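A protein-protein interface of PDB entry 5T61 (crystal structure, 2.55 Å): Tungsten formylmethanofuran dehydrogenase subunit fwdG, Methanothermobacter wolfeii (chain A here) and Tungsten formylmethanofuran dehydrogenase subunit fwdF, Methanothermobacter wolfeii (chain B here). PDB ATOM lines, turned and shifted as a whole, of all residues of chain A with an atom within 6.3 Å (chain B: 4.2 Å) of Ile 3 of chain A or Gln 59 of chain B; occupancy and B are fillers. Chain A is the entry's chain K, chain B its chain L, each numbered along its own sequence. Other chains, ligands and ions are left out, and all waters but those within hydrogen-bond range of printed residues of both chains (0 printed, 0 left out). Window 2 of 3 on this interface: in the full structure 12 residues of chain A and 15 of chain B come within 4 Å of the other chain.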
ATOM      1  N   ALA A   2      -4.787 -12.496   9.733  1.00  0.00           N
ATOM      2  CA  ALA A   2      -5.248 -13.648   8.965  1.00  0.00           C
ATOM      3  C   ALA A   2      -6.614 -14.104   9.460  1.00  0.00           C
ATOM      4  O   ALA A   2      -7.062 -13.699  10.537  1.00  0.00           O
ATOM      5  CB  ALA A   2      -4.245 -14.788   9.050  1.00  0.00           C
ATOM      6  N   ILE A   3      -7.303 -14.885   8.631  1.00  0.00           N
ATOM      7  CA  ILE A   3      -8.551 -15.521   9.038  1.00  0.00           C
ATOM      8  C   ILE A   3      -8.242 -16.650  10.013  1.00  0.00           C
ATOM      9  O   ILE A   3      -7.351 -17.474   9.769  1.00  0.00           O
ATOM     10  CB  ILE A   3      -9.323 -16.032   7.810  1.00  0.00           C
ATOM     11  CG1 ILE A   3      -9.984 -14.858   7.086  1.00  0.00           C
ATOM     12  CG2 ILE A   3     -10.340 -17.097   8.203  1.00  0.00           C
ATOM     13  CD1 ILE A   3     -10.633 -15.226   5.777  1.00  0.00           C
ATOM     14  N   GLY A   4      -8.992 -16.708  11.114  1.00  0.00           N
ATOM     15  CA  GLY A   4      -8.786 -17.739  12.111  1.00  0.00           C
ATOM     16  C   GLY A   4     -10.061 -18.013  12.881  1.00  0.00           C
ATOM     17  O   GLY A   4     -11.072 -17.322  12.725  1.00  0.00           O
ATOM     18  N   LEU A   5      -9.994 -19.041  13.723  1.00  0.00           N
ATOM     19  CA  LEU A   5     -11.132 -19.424  14.551  1.00  0.00           C
ATOM     20  C   LEU A   5     -11.224 -18.516  15.782  1.00  0.00           C
ATOM     21  O   LEU A   5     -10.219 -18.278  16.468  1.00  0.00           O
ATOM     22  CB  LEU A   5     -11.036 -20.896  14.947  1.00  0.00           C
ATOM     23  CG  LEU A   5     -12.351 -21.591  15.320  1.00  0.00           C
ATOM     24  CD1 LEU A   5     -13.314 -21.604  14.144  1.00  0.00           C
ATOM     25  CD2 LEU A   5     -12.062 -23.015  15.756  1.00  0.00           C
ATOM     26  N   LYS A  63      -9.354 -24.132   9.054  1.00  0.00           N
ATOM     27  CA  LYS A  63     -10.330 -23.143   8.587  1.00  0.00           C
ATOM     28  C   LYS A  63     -11.149 -23.667   7.408  1.00  0.00           C
ATOM     29  O   LYS A  63     -11.309 -22.995   6.388  1.00  0.00           O
ATOM     30  CB  LYS A  63      -9.659 -21.815   8.218  1.00  0.00           C
ATOM     31  CG  LYS A  63      -8.838 -21.149   9.316  1.00  0.00           C
ATOM     32  CD  LYS A  63      -7.374 -21.543   9.234  1.00  0.00           C
ATOM     33  CE  LYS A  63      -6.567 -20.883  10.337  1.00  0.00           C
ATOM     34  NZ  LYS A  63      -5.105 -21.124  10.179  1.00  0.00           N
ATOM     35  N   LEU A  78     -15.149 -17.974  11.662  1.00  0.00           N
ATOM     36  CA  LEU A  78     -13.886 -17.744  10.974  1.00  0.00           C
ATOM     37  C   LEU A  78     -13.852 -16.274  10.573  1.00  0.00           C
ATOM     38  O   LEU A  78     -14.644 -15.841   9.729  1.00  0.00           O
ATOM     39  CB  LEU A  78     -13.753 -18.650   9.754  1.00  0.00           C
ATOM     40  CG  LEU A  78     -13.663 -20.138  10.079  1.00  0.00           C
ATOM     41  CD1 LEU A  78     -13.780 -20.957   8.809  1.00  0.00           C
ATOM     42  CD2 LEU A  78     -12.369 -20.442  10.818  1.00  0.00           C
ATOM     43  N   GLU A  79     -12.957 -15.508  11.188  1.00  0.00           N
ATOM     44  CA  GLU A  79     -12.848 -14.084  10.909  1.00  0.00           C
ATOM     45  C   GLU A  79     -11.405 -13.637  11.106  1.00  0.00           C
ATOM     46  O   GLU A  79     -10.525 -14.432  11.461  1.00  0.00           O
ATOM     47  CB  GLU A  79     -13.826 -13.274  11.764  1.00  0.00           C
ATOM     48  CG  GLU A  79     -13.975 -13.749  13.195  1.00  0.00           C
ATOM     49  CD  GLU A  79     -14.854 -12.818  14.005  1.00  0.00           C
ATOM     50  OE1 GLU A  79     -15.012 -13.050  15.218  1.00  0.00           O
ATOM     51  OE2 GLU A  79     -15.455 -11.901  13.405  1.00  0.00           O
ATOM     52  N   GLU A  80     -11.174 -12.343  10.865  1.00  0.00           N
ATOM     53  CA  GLU A  80      -9.852 -11.757  11.049  1.00  0.00           C
ATOM     54  C   GLU A  80      -9.404 -11.904  12.494  1.00  0.00           C
ATOM     55  O   GLU A  80     -10.145 -11.570  13.427  1.00  0.00           O
ATOM     56  CB  GLU A  80      -9.845 -10.269  10.683  1.00  0.00           C
ATOM     57  CG  GLU A  80      -9.025  -9.916   9.486  1.00  0.00           C
ATOM     58  CD  GLU A  80      -7.575 -10.343   9.582  1.00  0.00           C
ATOM     59  OE1 GLU A  80      -7.001 -10.693   8.527  1.00  0.00           O
ATOM     60  OE2 GLU A  80      -7.019 -10.370  10.692  1.00  0.00           O
ATOM     61  N   LEU A  81      -8.186 -12.411  12.666  1.00  0.00           N
ATOM     62  CA  LEU A  81      -7.579 -12.597  13.974  1.00  0.00           C
ATOM     63  C   LEU A  81      -8.331 -13.695  14.712  1.00  0.00           C
ATOM     64  O   LEU A  81      -8.105 -14.881  14.470  1.00  0.00           O
ATOM     65  CB  LEU A  81      -7.580 -11.284  14.778  1.00  0.00           C
ATOM     66  CG  LEU A  81      -7.044 -10.012  14.107  1.00  0.00           C
ATOM     67  CD1 LEU A  81      -6.799  -8.924  15.138  1.00  0.00           C
ATOM     68  CD2 LEU A  81      -5.766 -10.317  13.357  1.00  0.00           C
ATOM     69  N   LYS B  10     -15.001  -6.712  -4.242  1.00  0.00           N
ATOM     70  CA  LYS B  10     -14.025  -7.745  -3.929  1.00  0.00           C
ATOM     71  C   LYS B  10     -12.990  -7.941  -5.031  1.00  0.00           C
ATOM     72  O   LYS B  10     -12.086  -8.769  -4.877  1.00  0.00           O
ATOM     73  CB  LYS B  10     -14.755  -9.061  -3.632  1.00  0.00           C
ATOM     74  CG  LYS B  10     -15.708  -8.929  -2.465  1.00  0.00           C
ATOM     75  CD  LYS B  10     -16.377 -10.236  -2.147  1.00  0.00           C
ATOM     76  CE  LYS B  10     -16.507 -10.335  -0.649  1.00  0.00           C
ATOM     77  NZ  LYS B  10     -16.502 -11.725  -0.136  1.00  0.00           N
ATOM     78  N   ALA B  53     -12.816 -21.871   4.028  1.00  0.00           N
ATOM     79  CA  ALA B  53     -13.479 -20.708   4.617  1.00  0.00           C
ATOM     80  C   ALA B  53     -14.074 -19.791   3.552  1.00  0.00           C
ATOM     81  O   ALA B  53     -15.189 -19.280   3.717  1.00  0.00           O
ATOM     82  CB  ALA B  53     -12.495 -19.936   5.494  1.00  0.00           C
ATOM     83  N   MET B  54     -13.344 -19.562   2.458  1.00  0.00           N
ATOM     84  CA  MET B  54     -13.826 -18.642   1.433  1.00  0.00           C
ATOM     85  C   MET B  54     -14.998 -19.220   0.648  1.00  0.00           C
ATOM     86  O   MET B  54     -15.761 -18.456   0.050  1.00  0.00           O
ATOM     87  CB  MET B  54     -12.691 -18.265   0.473  1.00  0.00           C
ATOM     88  CG  MET B  54     -11.505 -17.584   1.138  1.00  0.00           C
ATOM     89  SD  MET B  54     -11.931 -16.145   2.139  1.00  0.00           S
ATOM     90  CE  MET B  54     -12.718 -15.087   0.925  1.00  0.00           C
ATOM     91  N   THR B  57     -18.196 -20.110   3.998  1.00  0.00           N
ATOM     92  CA  THR B  57     -18.602 -19.091   4.955  1.00  0.00           C
ATOM     93  C   THR B  57     -18.654 -17.717   4.304  1.00  0.00           C
ATOM     94  O   THR B  57     -18.047 -17.469   3.257  1.00  0.00           O
ATOM     95  CB  THR B  57     -17.654 -19.043   6.165  1.00  0.00           C
ATOM     96  OG1 THR B  57     -16.351 -18.618   5.742  1.00  0.00           O
ATOM     97  CG2 THR B  57     -17.572 -20.397   6.857  1.00  0.00           C
ATOM     98  N   GLU B  58     -19.426 -16.831   4.931  1.00  0.00           N
ATOM     99  CA  GLU B  58     -19.479 -15.440   4.512  1.00  0.00           C
ATOM    100  C   GLU B  58     -18.239 -14.700   4.988  1.00  0.00           C
ATOM    101  O   GLU B  58     -17.877 -14.758   6.167  1.00  0.00           O
ATOM    102  CB  GLU B  58     -20.733 -14.755   5.050  1.00  0.00           C
ATOM    103  CG  GLU B  58     -22.013 -15.201   4.384  1.00  0.00           C
ATOM    104  CD  GLU B  58     -22.752 -14.036   3.753  1.00  0.00           C
ATOM    105  OE1 GLU B  58     -23.598 -13.422   4.438  1.00  0.00           O
ATOM    106  OE2 GLU B  58     -22.467 -13.721   2.577  1.00  0.00           O
ATOM    107  N   GLN B  59     -17.605 -13.989   4.065  1.00  0.00           N
ATOM    108  CA  GLN B  59     -16.402 -13.223   4.338  1.00  0.00           C
ATOM    109  C   GLN B  59     -16.485 -11.951   3.516  1.00  0.00           C
ATOM    110  O   GLN B  59     -16.986 -11.970   2.389  1.00  0.00           O
ATOM    111  CB  GLN B  59     -15.127 -13.993   3.961  1.00  0.00           C
ATOM    112  CG  GLN B  59     -14.956 -15.350   4.628  1.00  0.00           C
ATOM    113  CD  GLN B  59     -14.665 -15.254   6.113  1.00  0.00           C
ATOM    114  OE1 GLN B  59     -14.092 -14.275   6.584  1.00  0.00           O
ATOM    115  NE2 GLN B  59     -15.057 -16.283   6.857  1.00  0.00           N
ATOM    116  N   GLU B  60     -16.009 -10.848   4.078  1.00  0.00           N
ATOM    117  CA  GLU B  60     -15.911  -9.614   3.310  1.00  0.00           C
ATOM    118  C   GLU B  60     -14.598  -9.514   2.560  1.00  0.00           C
ATOM    119  O   GLU B  60     -14.512  -8.770   1.575  1.00  0.00           O
ATOM    120  CB  GLU B  60     -16.083  -8.408   4.233  1.00  0.00           C
ATOM    121  CG  GLU B  60     -17.196  -8.611   5.246  1.00  0.00           C
ATOM    122  CD  GLU B  60     -16.972  -7.819   6.506  1.00  0.00           C
ATOM    123  OE1 GLU B  60     -17.365  -8.290   7.584  1.00  0.00           O
ATOM    124  OE2 GLU B  60     -16.419  -6.709   6.421  1.00  0.00           O
ATOM    125  N   LYS B  61     -13.583 -10.257   2.994  1.00  0.00           N
ATOM    126  CA  LYS B  61     -12.288 -10.193   2.338  1.00  0.00           C
ATOM    127  C   LYS B  61     -12.351 -10.834   0.966  1.00  0.00           C
ATOM    128  O   LYS B  61     -13.151 -11.741   0.717  1.00  0.00           O
ATOM    129  CB  LYS B  61     -11.234 -10.897   3.164  1.00  0.00           C
ATOM    130  CG  LYS B  61     -11.175 -10.361   4.553  1.00  0.00           C
ATOM    131  CD  LYS B  61      -9.990 -10.963   5.149  1.00  0.00           C
ATOM    132  CE  LYS B  61      -9.346 -10.000   6.057  1.00  0.00           C
ATOM    133  NZ  LYS B  61      -8.322 -10.850   6.654  1.00  0.00           N
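The side-chain amide nitrogen (NE2) of Gln 59 of chain B lies within hydrogen-bond range of the backbone carbonyl oxygen (O) of Leu 78 of chain A (2.9 Å).
The backbone NH (N) of Ala 53 of chain B is in hydrogen-bond range of the backbone carbonyl oxygen (O) of Lys 63 of chain A (3.0 Å).
OE1 of Glu 80 of chain A sits close to NZ of Lys 61 of chain B, at 2.3 Å.
NZ of Lys 10 of chain B sits at hydrogen-bond distance from O of Lys 61 of chain B, 3.5 Å away.
O of Ala 53 of chain B lies within hydrogen-bond range of OG1 of Thr 57 of chain B, at 2.4 Å.
NZ of Lys 10 of chain B sits at hydrogen-bond distance from O of Gln 59 of chain B, 2.6 Å away.
N of Ala 2 of chain A is in hydrogen-bond range of OE1 of Glu 80 of chain A, 3.1 Å away.
NE2 of Gln 59 of chain B sits at hydrogen-bond distance from OG1 of Thr 57 of chain B, 2.9 Å away.
Among the printed residues, merely in contact across the chains: Ile 3 of chain A with Met 54 of chain B (3.97 Å), Ile 3 of chain A with Gln 59 of chain B (3.7 Å) and Leu 78 of chain A with Ala 53 of chain B (3.7 Å).
Of chain B, only Met 54 (3.97 Å) and Gln 59 (3.7 Å) come within 4 Å of Ile 3 of chain A.
Gln 59 of chain B touches just these residues of chain A: Ile 3 and Leu 78.
Of the printed residues of chain B, Lys 63 of chain A touches Ala 53 (3.0 Å).
Of the printed residues of chain B, Leu 78 of chain A touches Ala 53 and Gln 59.
Of the printed residues of chain A, Met 54 of chain B touches Ile 3 (3.97 Å).
Ala 2 of chain A touches none of the printed residues of chain B.
Glu 58 of chain B touches none of the printed residues of chain A.
The nearest residue of chain A that does not touch Gln 59 of chain B is Glu 79 of chain A (4.5 Å).
Of the 8 printed residues of chain B, 4 touch a printed residue of chain A.
Hydrophobic or aromatic side chains of chain B within 4 Å of the printed part of chain A: Ala 53 and Met 54.
Of the 9 printed residues of chain A, 4 touch a printed residue of chain B.
Among the printed residues, Asp or Glu carboxylates within 4 Å of a Lys or Arg side-chain nitrogen of the other chain: Glu 80 of chain A with Lys 61 of chain B (2.3 Å).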
